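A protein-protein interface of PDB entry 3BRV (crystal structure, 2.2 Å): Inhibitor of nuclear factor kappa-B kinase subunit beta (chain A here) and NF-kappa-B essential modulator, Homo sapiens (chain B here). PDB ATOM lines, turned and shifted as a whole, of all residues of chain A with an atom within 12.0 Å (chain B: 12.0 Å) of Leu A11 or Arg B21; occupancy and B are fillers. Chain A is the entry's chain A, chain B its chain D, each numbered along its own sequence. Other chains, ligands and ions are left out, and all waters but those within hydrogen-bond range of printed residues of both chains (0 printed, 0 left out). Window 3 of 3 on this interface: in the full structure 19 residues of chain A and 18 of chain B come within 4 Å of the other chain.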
ATOM      1  N   SER A   8      -5.966   4.691  11.494  1.00  0.00           N
ATOM      2  CA  SER A   8      -5.362   5.924  12.163  1.00  0.00           C
ATOM      3  C   SER A   8      -3.850   6.184  11.924  1.00  0.00           C
ATOM      4  O   SER A   8      -2.953   5.361  12.176  1.00  0.00           O
ATOM      5  CB  SER A   8      -5.686   6.004  13.670  1.00  0.00           C
ATOM      6  OG  SER A   8      -4.733   6.833  14.356  1.00  0.00           O
ATOM      7  N   GLU A   9      -3.603   7.396  11.479  1.00  0.00           N
ATOM      8  CA  GLU A   9      -2.324   7.876  10.979  1.00  0.00           C
ATOM      9  C   GLU A   9      -1.218   7.854  12.039  1.00  0.00           C
ATOM     10  O   GLU A   9      -0.067   7.551  11.738  1.00  0.00           O
ATOM     11  CB  GLU A   9      -2.583   9.300  10.423  1.00  0.00           C
ATOM     12  N   GLU A  10      -1.599   8.157  13.287  1.00  0.00           N
ATOM     13  CA  GLU A  10      -0.706   8.166  14.463  1.00  0.00           C
ATOM     14  C   GLU A  10      -0.314   6.775  14.916  1.00  0.00           C
ATOM     15  O   GLU A  10       0.849   6.513  15.171  1.00  0.00           O
ATOM     16  CB  GLU A  10      -1.315   8.933  15.641  1.00  0.00           C
ATOM     17  CG  GLU A  10      -0.721  10.327  15.805  1.00  0.00           C
ATOM     18  CD  GLU A  10      -0.972  10.935  17.188  1.00  0.00           C
ATOM     19  OE1 GLU A  10      -0.616  10.266  18.183  1.00  0.00           O
ATOM     20  OE2 GLU A  10      -1.501  12.070  17.287  1.00  0.00           O
ATOM     21  N   LEU A  11      -1.267   5.876  15.028  1.00  0.00           N
ATOM     22  CA  LEU A  11      -0.922   4.522  15.382  1.00  0.00           C
ATOM     23  C   LEU A  11       0.123   3.955  14.406  1.00  0.00           C
ATOM     24  O   LEU A  11       0.983   3.162  14.814  1.00  0.00           O
ATOM     25  CB  LEU A  11      -2.154   3.601  15.312  1.00  0.00           C
ATOM     26  CG  LEU A  11      -3.142   3.607  16.451  1.00  0.00           C
ATOM     27  CD1 LEU A  11      -4.293   2.700  16.022  1.00  0.00           C
ATOM     28  CD2 LEU A  11      -2.563   3.227  17.781  1.00  0.00           C
ATOM     29  N   VAL A  12      -0.052   4.300  13.131  1.00  0.00           N
ATOM     30  CA  VAL A  12       0.778   3.843  11.988  1.00  0.00           C
ATOM     31  C   VAL A  12       2.193   4.473  12.018  1.00  0.00           C
ATOM     32  O   VAL A  12       3.174   3.788  11.781  1.00  0.00           O
ATOM     33  CB  VAL A  12       0.047   4.146  10.662  1.00  0.00           C
ATOM     34  CG1 VAL A  12       0.993   4.235   9.453  1.00  0.00           C
ATOM     35  CG2 VAL A  12      -0.947   3.053  10.374  1.00  0.00           C
ATOM     36  N   ALA A  13       2.262   5.767  12.328  1.00  0.00           N
ATOM     37  CA  ALA A  13       3.491   6.518  12.536  1.00  0.00           C
ATOM     38  C   ALA A  13       4.247   5.997  13.756  1.00  0.00           C
ATOM     39  O   ALA A  13       5.439   5.840  13.729  1.00  0.00           O
ATOM     40  CB  ALA A  13       3.129   8.041  12.724  1.00  0.00           C
ATOM     41  N   GLU A  14       3.554   5.739  14.845  1.00  0.00           N
ATOM     42  CA  GLU A  14       4.203   5.204  16.005  1.00  0.00           C
ATOM     43  C   GLU A  14       4.811   3.868  15.745  1.00  0.00           C
ATOM     44  O   GLU A  14       5.914   3.558  16.279  1.00  0.00           O
ATOM     45  CB  GLU A  14       3.200   5.014  17.101  1.00  0.00           C
ATOM     46  CG  GLU A  14       3.813   5.100  18.422  1.00  0.00           C
ATOM     47  CD  GLU A  14       2.803   4.719  19.479  1.00  0.00           C
ATOM     48  OE1 GLU A  14       1.688   4.217  19.086  1.00  0.00           O
ATOM     49  OE2 GLU A  14       3.132   4.893  20.672  1.00  0.00           O
ATOM     50  N   ALA A  15       4.116   3.069  14.930  1.00  0.00           N
ATOM     51  CA  ALA A  15       4.573   1.730  14.727  1.00  0.00           C
ATOM     52  C   ALA A  15       5.885   1.747  13.955  1.00  0.00           C
ATOM     53  O   ALA A  15       6.809   1.039  14.329  1.00  0.00           O
ATOM     54  CB  ALA A  15       3.491   0.840  14.064  1.00  0.00           C
ATOM     55  N   HIS A  16       5.948   2.537  12.895  1.00  0.00           N
ATOM     56  CA  HIS A  16       7.165   2.793  12.147  1.00  0.00           C
ATOM     57  C   HIS A  16       8.259   3.271  13.056  1.00  0.00           C
ATOM     58  O   HIS A  16       9.377   2.817  12.951  1.00  0.00           O
ATOM     59  CB  HIS A  16       6.888   3.852  11.084  1.00  0.00           C
ATOM     60  CG  HIS A  16       8.077   4.263  10.283  1.00  0.00           C
ATOM     61  ND1 HIS A  16       8.825   3.379   9.531  1.00  0.00           N
ATOM     62  CD2 HIS A  16       8.627   5.489  10.082  1.00  0.00           C
ATOM     63  CE1 HIS A  16       9.786   4.021   8.910  1.00  0.00           C
ATOM     64  NE2 HIS A  16       9.688   5.314   9.222  1.00  0.00           N
ATOM     65  N   ASN A  17       7.953   4.221  13.926  1.00  0.00           N
ATOM     66  CA  ASN A  17       8.951   4.686  14.881  1.00  0.00           C
ATOM     67  C   ASN A  17       9.523   3.584  15.812  1.00  0.00           C
ATOM     68  O   ASN A  17      10.717   3.528  16.002  1.00  0.00           O
ATOM     69  CB  ASN A  17       8.421   5.893  15.640  1.00  0.00           C
ATOM     70  CG  ASN A  17       8.586   7.198  14.852  1.00  0.00           C
ATOM     71  OD1 ASN A  17       8.906   7.193  13.639  1.00  0.00           O
ATOM     72  ND2 ASN A  17       8.437   8.339  15.555  1.00  0.00           N
ATOM     73  N   LEU A  18       8.658   2.713  16.365  1.00  0.00           N
ATOM     74  CA  LEU A  18       9.045   1.584  17.248  1.00  0.00           C
ATOM     75  C   LEU A  18       9.818   0.456  16.553  1.00  0.00           C
ATOM     76  O   LEU A  18      10.721  -0.115  17.142  1.00  0.00           O
ATOM     77  CB  LEU A  18       7.821   0.991  17.988  1.00  0.00           C
ATOM     78  CG  LEU A  18       7.254   2.077  18.933  1.00  0.00           C
ATOM     79  CD1 LEU A  18       5.900   1.665  19.412  1.00  0.00           C
ATOM     80  CD2 LEU A  18       8.196   2.354  20.110  1.00  0.00           C
ATOM     81  N   CYS A  19       9.461   0.204  15.305  1.00  0.00           N
ATOM     82  CA  CYS A  19      10.179  -0.717  14.428  1.00  0.00           C
ATOM     83  C   CYS A  19      11.581  -0.255  14.116  1.00  0.00           C
ATOM     84  O   CYS A  19      12.468  -1.093  13.938  1.00  0.00           O
ATOM     85  CB  CYS A  19       9.392  -1.003  13.103  1.00  0.00           C
ATOM     86  SG  CYS A  19       7.870  -2.064  13.368  1.00  0.00           S
ATOM     87  N   THR A  20      11.754   1.050  13.986  1.00  0.00           N
ATOM     88  CA  THR A  20      13.026   1.601  13.668  1.00  0.00           C
ATOM     89  C   THR A  20      13.947   1.409  14.896  1.00  0.00           C
ATOM     90  O   THR A  20      15.058   0.852  14.733  1.00  0.00           O
ATOM     91  CB  THR A  20      12.912   3.066  13.243  1.00  0.00           C
ATOM     92  OG1 THR A  20      12.122   3.161  12.061  1.00  0.00           O
ATOM     93  CG2 THR A  20      14.296   3.685  12.941  1.00  0.00           C
ATOM     94  N   LEU B  10     -19.851  -1.285   3.777  1.00  0.00           N
ATOM     95  CA  LEU B  10     -19.310  -0.278   4.708  1.00  0.00           C
ATOM     96  C   LEU B  10     -19.214  -0.759   6.178  1.00  0.00           C
ATOM     97  O   LEU B  10     -18.218  -0.514   6.848  1.00  0.00           O
ATOM     98  CB  LEU B  10     -20.040   1.052   4.619  1.00  0.00           C
ATOM     99  CG  LEU B  10     -19.476   2.257   5.425  1.00  0.00           C
ATOM    100  CD1 LEU B  10     -18.081   2.474   5.090  1.00  0.00           C
ATOM    101  CD2 LEU B  10     -20.327   3.600   5.236  1.00  0.00           C
ATOM    102  N   GLN B  11     -20.220  -1.452   6.683  1.00  0.00           N
ATOM    103  CA  GLN B  11     -20.159  -2.010   8.009  1.00  0.00           C
ATOM    104  C   GLN B  11     -18.967  -3.000   8.190  1.00  0.00           C
ATOM    105  O   GLN B  11     -18.236  -2.888   9.190  1.00  0.00           O
ATOM    106  CB  GLN B  11     -21.547  -2.625   8.416  1.00  0.00           C
ATOM    107  CG  GLN B  11     -21.572  -3.437   9.713  1.00  0.00           C
ATOM    108  CD  GLN B  11     -21.122  -2.645  10.945  1.00  0.00           C
ATOM    109  OE1 GLN B  11     -21.118  -1.429  10.913  1.00  0.00           O
ATOM    110  NE2 GLN B  11     -20.764  -3.324  12.022  1.00  0.00           N
ATOM    111  N   ARG B  12     -18.814  -3.978   7.268  1.00  0.00           N
ATOM    112  CA  ARG B  12     -17.681  -4.909   7.275  1.00  0.00           C
ATOM    113  C   ARG B  12     -16.341  -4.190   7.313  1.00  0.00           C
ATOM    114  O   ARG B  12     -15.454  -4.591   8.080  1.00  0.00           O
ATOM    115  CB  ARG B  12     -17.737  -5.926   6.121  1.00  0.00           C
ATOM    116  N   CYS B  13     -16.191  -3.114   6.530  1.00  0.00           N
ATOM    117  CA  CYS B  13     -14.975  -2.245   6.550  1.00  0.00           C
ATOM    118  C   CYS B  13     -14.638  -1.493   7.857  1.00  0.00           C
ATOM    119  O   CYS B  13     -13.490  -1.389   8.248  1.00  0.00           O
ATOM    120  CB  CYS B  13     -15.079  -1.240   5.409  1.00  0.00           C
ATOM    121  SG  CYS B  13     -13.465  -0.608   4.965  1.00  0.00           S
ATOM    122  N   LEU B  14     -15.639  -0.921   8.534  1.00  0.00           N
ATOM    123  CA  LEU B  14     -15.436  -0.128   9.755  1.00  0.00           C
ATOM    124  C   LEU B  14     -15.101  -1.106  10.845  1.00  0.00           C
ATOM    125  O   LEU B  14     -14.389  -0.799  11.752  1.00  0.00           O
ATOM    126  CB  LEU B  14     -16.683   0.653  10.152  1.00  0.00           C
ATOM    127  CG  LEU B  14     -17.259   1.640   9.134  1.00  0.00           C
ATOM    128  CD1 LEU B  14     -18.668   2.086   9.496  1.00  0.00           C
ATOM    129  CD2 LEU B  14     -16.368   2.832   9.110  1.00  0.00           C
ATOM    130  N   GLU B  15     -15.680  -2.292  10.771  1.00  0.00           N
ATOM    131  CA  GLU B  15     -15.394  -3.345  11.712  1.00  0.00           C
ATOM    132  C   GLU B  15     -13.988  -3.959  11.531  1.00  0.00           C
ATOM    133  O   GLU B  15     -13.269  -4.255  12.528  1.00  0.00           O
ATOM    134  CB  GLU B  15     -16.452  -4.418  11.583  1.00  0.00           C
ATOM    135  CG  GLU B  15     -16.613  -5.273  12.753  1.00  0.00           C
ATOM    136  CD  GLU B  15     -17.907  -6.074  12.683  1.00  0.00           C
ATOM    137  OE1 GLU B  15     -17.923  -7.112  13.406  1.00  0.00           O
ATOM    138  OE2 GLU B  15     -18.871  -5.670  11.934  1.00  0.00           O
ATOM    139  N   GLU B  16     -13.569  -4.135  10.294  1.00  0.00           N
ATOM    140  CA  GLU B  16     -12.186  -4.499  10.027  1.00  0.00           C
ATOM    141  C   GLU B  16     -11.224  -3.368  10.413  1.00  0.00           C
ATOM    142  O   GLU B  16     -10.150  -3.657  10.853  1.00  0.00           O
ATOM    143  CB  GLU B  16     -12.007  -4.812   8.563  1.00  0.00           C
ATOM    144  CG  GLU B  16     -12.201  -6.277   8.218  1.00  0.00           C
ATOM    145  CD  GLU B  16     -11.544  -6.671   6.904  1.00  0.00           C
ATOM    146  OE1 GLU B  16     -10.480  -6.089   6.566  1.00  0.00           O
ATOM    147  OE2 GLU B  16     -12.104  -7.562   6.214  1.00  0.00           O
ATOM    148  N   ASN B  17     -11.590  -2.090  10.247  1.00  0.00           N
ATOM    149  CA  ASN B  17     -10.639  -1.031  10.539  1.00  0.00           C
ATOM    150  C   ASN B  17     -10.353  -0.976  12.027  1.00  0.00           C
ATOM    151  O   ASN B  17      -9.196  -0.783  12.427  1.00  0.00           O
ATOM    152  CB  ASN B  17     -11.040   0.330  10.019  1.00  0.00           C
ATOM    153  CG  ASN B  17     -10.830   0.482   8.511  1.00  0.00           C
ATOM    154  OD1 ASN B  17     -10.182  -0.349   7.822  1.00  0.00           O
ATOM    155  ND2 ASN B  17     -11.443   1.538   7.968  1.00  0.00           N
ATOM    156  N   GLN B  18     -11.384  -1.277  12.834  1.00  0.00           N
ATOM    157  CA  GLN B  18     -11.276  -1.195  14.241  1.00  0.00           C
ATOM    158  C   GLN B  18     -10.411  -2.366  14.698  1.00  0.00           C
ATOM    159  O   GLN B  18      -9.532  -2.165  15.584  1.00  0.00           O
ATOM    160  CB  GLN B  18     -12.674  -1.266  14.911  1.00  0.00           C
ATOM    161  CG  GLN B  18     -12.450  -1.594  16.348  1.00  0.00           C
ATOM    162  CD  GLN B  18     -13.566  -1.315  17.312  1.00  0.00           C
ATOM    163  OE1 GLN B  18     -13.340  -0.694  18.350  1.00  0.00           O
ATOM    164  NE2 GLN B  18     -14.713  -1.862  17.066  1.00  0.00           N
ATOM    165  N   GLU B  19     -10.622  -3.573  14.120  1.00  0.00           N
ATOM    166  CA  GLU B  19      -9.782  -4.748  14.443  1.00  0.00           C
ATOM    167  C   GLU B  19      -8.305  -4.466  14.120  1.00  0.00           C
ATOM    168  O   GLU B  19      -7.454  -4.700  14.928  1.00  0.00           O
ATOM    169  CB  GLU B  19     -10.305  -6.042  13.803  1.00  0.00           C
ATOM    170  CG  GLU B  19     -11.801  -6.247  14.142  1.00  0.00           C
ATOM    171  CD  GLU B  19     -12.590  -7.399  13.412  1.00  0.00           C
ATOM    172  OE1 GLU B  19     -12.981  -8.374  14.098  1.00  0.00           O
ATOM    173  OE2 GLU B  19     -12.934  -7.301  12.187  1.00  0.00           O
ATOM    174  N   LEU B  20      -8.007  -3.888  12.959  1.00  0.00           N
ATOM    175  CA  LEU B  20      -6.629  -3.620  12.536  1.00  0.00           C
ATOM    176  C   LEU B  20      -5.973  -2.584  13.443  1.00  0.00           C
ATOM    177  O   LEU B  20      -4.797  -2.695  13.794  1.00  0.00           O
ATOM    178  CB  LEU B  20      -6.567  -3.166  11.064  1.00  0.00           C
ATOM    179  CG  LEU B  20      -6.962  -4.187  10.006  1.00  0.00           C
ATOM    180  CD1 LEU B  20      -7.155  -3.628   8.562  1.00  0.00           C
ATOM    181  CD2 LEU B  20      -6.102  -5.449  10.022  1.00  0.00           C
ATOM    182  N   ARG B  21      -6.748  -1.586  13.813  1.00  0.00           N
ATOM    183  CA  ARG B  21      -6.299  -0.467  14.674  1.00  0.00           C
ATOM    184  C   ARG B  21      -5.940  -0.963  16.042  1.00  0.00           C
ATOM    185  O   ARG B  21      -4.926  -0.573  16.576  1.00  0.00           O
ATOM    186  CB  ARG B  21      -7.454   0.564  14.869  1.00  0.00           C
ATOM    187  CG  ARG B  21      -7.331   1.899  14.203  1.00  0.00           C
ATOM    188  CD  ARG B  21      -8.499   2.844  14.670  1.00  0.00           C
ATOM    189  NE  ARG B  21      -9.341   3.048  13.508  1.00  0.00           N
ATOM    190  CZ  ARG B  21     -10.619   2.712  13.300  1.00  0.00           C
ATOM    191  NH1 ARG B  21     -11.441   2.182  14.225  1.00  0.00           N
ATOM    192  NH2 ARG B  21     -11.084   2.971  12.086  1.00  0.00           N
ATOM    193  N   ASP B  22      -6.859  -1.742  16.622  1.00  0.00           N
ATOM    194  CA  ASP B  22      -6.615  -2.525  17.812  1.00  0.00           C
ATOM    195  C   ASP B  22      -5.321  -3.390  17.674  1.00  0.00           C
ATOM    196  O   ASP B  22      -4.507  -3.346  18.552  1.00  0.00           O
ATOM    197  CB  ASP B  22      -7.866  -3.367  18.219  1.00  0.00           C
ATOM    198  CG  ASP B  22      -9.104  -2.489  18.666  1.00  0.00           C
ATOM    199  OD1 ASP B  22      -9.113  -1.206  18.635  1.00  0.00           O
ATOM    200  OD2 ASP B  22     -10.126  -3.119  19.109  1.00  0.00           O
ATOM    201  N   ALA B  23      -5.100  -4.139  16.591  1.00  0.00           N
ATOM    202  CA  ALA B  23      -3.898  -4.969  16.518  1.00  0.00           C
ATOM    203  C   ALA B  23      -2.630  -4.126  16.600  1.00  0.00           C
ATOM    204  O   ALA B  23      -1.716  -4.474  17.384  1.00  0.00           O
ATOM    205  CB  ALA B  23      -3.863  -5.941  15.260  1.00  0.00           C
ATOM    206  N   ILE B  24      -2.556  -3.059  15.776  1.00  0.00           N
ATOM    207  CA  ILE B  24      -1.408  -2.122  15.804  1.00  0.00           C
ATOM    208  C   ILE B  24      -1.276  -1.440  17.174  1.00  0.00           C
ATOM    209  O   ILE B  24      -0.203  -1.271  17.668  1.00  0.00           O
ATOM    210  CB  ILE B  24      -1.498  -1.049  14.719  1.00  0.00           C
ATOM    211  CG1 ILE B  24      -1.452  -1.690  13.316  1.00  0.00           C
ATOM    212  CG2 ILE B  24      -0.322   0.046  14.853  1.00  0.00           C
ATOM    213  CD1 ILE B  24      -2.287  -0.956  12.311  1.00  0.00           C
ATOM    214  N   ARG B  25      -2.351  -1.019  17.789  1.00  0.00           N
ATOM    215  CA  ARG B  25      -2.210  -0.424  19.116  1.00  0.00           C
ATOM    216  C   ARG B  25      -1.599  -1.418  20.146  1.00  0.00           C
ATOM    217  O   ARG B  25      -0.741  -1.051  20.916  1.00  0.00           O
ATOM    218  CB  ARG B  25      -3.562   0.138  19.575  1.00  0.00           C
ATOM    219  CG  ARG B  25      -3.541   0.857  20.941  1.00  0.00           C
ATOM    220  CD  ARG B  25      -4.664   1.896  20.883  1.00  0.00           C
ATOM    221  NE  ARG B  25      -5.864   1.277  20.339  1.00  0.00           N
ATOM    222  CZ  ARG B  25      -6.718   1.858  19.503  1.00  0.00           C
ATOM    223  NH1 ARG B  25      -6.518   3.105  19.063  1.00  0.00           N
ATOM    224  NH2 ARG B  25      -7.765   1.163  19.092  1.00  0.00           N
ATOM    225  N   GLN B  26      -2.032  -2.683  20.143  1.00  0.00           N
ATOM    226  CA  GLN B  26      -1.468  -3.720  21.027  1.00  0.00           C
ATOM    227  C   GLN B  26      -0.021  -3.972  20.700  1.00  0.00           C
ATOM    228  O   GLN B  26       0.839  -4.072  21.597  1.00  0.00           O
ATOM    229  CB  GLN B  26      -2.201  -5.050  20.837  1.00  0.00           C
ATOM    230  CG  GLN B  26      -3.285  -5.333  21.862  1.00  0.00           C
ATOM    231  CD  GLN B  26      -4.296  -4.201  21.953  1.00  0.00           C
ATOM    232  OE1 GLN B  26      -4.457  -3.599  23.009  1.00  0.00           O
ATOM    233  NE2 GLN B  26      -4.985  -3.906  20.847  1.00  0.00           N
ATOM    234  N   SER B  27       0.205  -4.130  19.400  1.00  0.00           N
ATOM    235  CA  SER B  27       1.483  -4.407  18.861  1.00  0.00           C
ATOM    236  C   SER B  27       2.532  -3.332  19.225  1.00  0.00           C
ATOM    237  O   SER B  27       3.726  -3.620  19.425  1.00  0.00           O
ATOM    238  CB  SER B  27       1.337  -4.496  17.350  1.00  0.00           C
ATOM    239  OG  SER B  27       2.642  -4.612  16.875  1.00  0.00           O
ATOM    240  N   ASN B  28       2.103  -2.087  19.267  1.00  0.00           N
ATOM    241  CA  ASN B  28       3.005  -0.973  19.582  1.00  0.00           C
ATOM    242  C   ASN B  28       3.447  -0.966  21.019  1.00  0.00           C
ATOM    243  O   ASN B  28       4.617  -0.743  21.286  1.00  0.00           O
ATOM    244  CB  ASN B  28       2.357   0.378  19.282  1.00  0.00           C
ATOM    245  CG  ASN B  28       2.390   0.743  17.810  1.00  0.00           C
ATOM    246  OD1 ASN B  28       1.632   1.584  17.388  1.00  0.00           O
ATOM    247  ND2 ASN B  28       3.260   0.143  17.047  1.00  0.00           N
ATOM    248  N   GLN B  29       2.491  -1.167  21.950  1.00  0.00           N
ATOM    249  CA  GLN B  29       2.826  -1.339  23.352  1.00  0.00           C
ATOM    250  C   GLN B  29       3.691  -2.574  23.519  1.00  0.00           C
ATOM    251  O   GLN B  29       4.586  -2.564  24.360  1.00  0.00           O
ATOM    252  CB  GLN B  29       1.575  -1.404  24.223  1.00  0.00           C
ATOM    253  N   ILE B  30       3.521  -3.622  22.700  1.00  0.00           N
ATOM    254  CA  ILE B  30       4.438  -4.749  22.853  1.00  0.00           C
ATOM    255  C   ILE B  30       5.852  -4.506  22.341  1.00  0.00           C
ATOM    256  O   ILE B  30       6.774  -4.907  22.986  1.00  0.00           O
ATOM    257  CB  ILE B  30       3.895  -6.174  22.468  1.00  0.00           C
ATOM    258  CG1 ILE B  30       4.244  -6.540  21.043  1.00  0.00           C
ATOM    259  CG2 ILE B  30       2.463  -6.429  22.924  1.00  0.00           C
ATOM    260  CD1 ILE B  30       5.632  -7.181  20.989  1.00  0.00           C
ATOM    261  N   LEU B  31       6.014  -3.826  21.209  1.00  0.00           N
ATOM    262  CA  LEU B  31       7.298  -3.411  20.677  1.00  0.00           C
ATOM    263  C   LEU B  31       8.110  -2.561  21.617  1.00  0.00           C
ATOM    264  O   LEU B  31       9.351  -2.741  21.670  1.00  0.00           O
ATOM    265  CB  LEU B  31       7.156  -2.621  19.364  1.00  0.00           C
ATOM    266  CG  LEU B  31       6.846  -3.459  18.130  1.00  0.00           C
ATOM    267  CD1 LEU B  31       6.511  -2.461  17.017  1.00  0.00           C
ATOM    268  CD2 LEU B  31       7.939  -4.467  17.713  1.00  0.00           C
ATOM    269  N   ARG B  32       7.453  -1.603  22.293  1.00  0.00           N
ATOM    270  CA  ARG B  32       8.170  -0.790  23.264  1.00  0.00           C
ATOM    271  C   ARG B  32       8.813  -1.658  24.401  1.00  0.00           C
ATOM    272  O   ARG B  32       9.948  -1.398  24.814  1.00  0.00           O
ATOM    273  CB  ARG B  32       7.229   0.226  23.888  1.00  0.00           C
ATOM    274  CG  ARG B  32       7.909   1.182  24.781  1.00  0.00           C
ATOM    275  CD  ARG B  32       7.003   2.281  25.199  1.00  0.00           C
ATOM    276  NE  ARG B  32       6.825   3.228  24.125  1.00  0.00           N
ATOM    277  CZ  ARG B  32       5.697   3.358  23.428  1.00  0.00           C
ATOM    278  NH1 ARG B  32       4.626   2.601  23.690  1.00  0.00           N
ATOM    279  NH2 ARG B  32       5.654   4.230  22.437  1.00  0.00           N
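No residue of chain B comes within 4 Å of Ser A8. No residue of chain B comes within 4 Å of Glu A9. No residue of chain B comes within 4 Å of Glu A10. Of chain B, only Arg B21 (3.4 Å), Ile B24 (3.4 Å), Arg B25 (3.7 Å) and Asn B28 (3.1 Å) come within 4 Å of Leu A11. No residue of chain B comes within 4 Å of Val A12. No residue of chain B comes within 4 Å of Ala A13. Of chain B, only Asn B28 (3.1 Å) and Arg B32 (3.1 Å) come within 4 Å of Glu A14. Ala A15 touches two residues of chain B. Of the printed residues of chain B, Cys A19 touches Leu B31. No residue of chain A comes within 4 Å of Asn B17. No residue of chain A comes within 4 Å of Gln B18. Glu B19 touches none of the printed residues of chain A. No residue of chain A comes within 4 Å of Leu B20. Arg B21 touches one residue of chain A. No residue of chain A comes within 4 Å of Ala B23. Printed residues of chain A within 4 Å of Ile B24: Leu A11 and Ala A15. Arg B25 touches just one residue of chain A: Leu A11 (3.7 Å). Ile B30 touches none of the printed residues of chain A. Of the printed residues of chain A, Leu B31 touches Leu A18 (3.8 Å) and Cys A19 (3.9 Å). Printed residues of chain A within 4 Å of Arg B32: Glu A14 (3.1 Å) and Leu A18 (3.9 Å). The nearest printed residue of chain B that does not touch Cys A19 is Asn B28 (6.3 Å).
Leu A11 touches Arg B21 (CD1 to O, 3.4 Å). CG2 of Ile B24 touches O of Leu A11, 3.4 Å away. Leu A11 touches Arg B25. Ala A15 touches Ile B24 (CB to CG2, 3.97 Å). ND2 of Asn B28 touches CB of Ala A15, 3.1 Å away. Leu A18 touches Asn B28 (CD1 to O, 3.3 Å). CD1 of Leu B31 touches CB of Leu A18, at 3.8 Å. Leu A18 touches Arg B32. Leu B31 touches Cys A19 (CD1 to SG, 3.9 Å).
The side-chain carboxylate of Glu A14 is in salt-bridge range of the guanidinium group of Arg B32 (3.1 Å). OD1 of Asn B28 lies close to O of Leu A11, 3.1 Å away. OD1 of Asn B28 sits close to OE1 of Glu A14, at 3.1 Å.
Hydrophobic or aromatic side chains of chain B that line the printed part of chain A: Ile B24 and Leu B31. Among the printed residues, 12 pairs touch across the chains.
The side-chain sulfur (SG) of Cys A19 sits at hydrogen-bond distance from the backbone carbonyl oxygen (O) of Ala A15 (3.4 Å). The backbone carbonyl oxygen of Ile B24 sits close to the side-chain amide oxygen of Asn B28 (3.4 Å). The side-chain carboxylate (OD1) of Asp B22 lies within salt-bridge range of the guanidinium group (NH2) of Arg B25 (2.8 Å).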
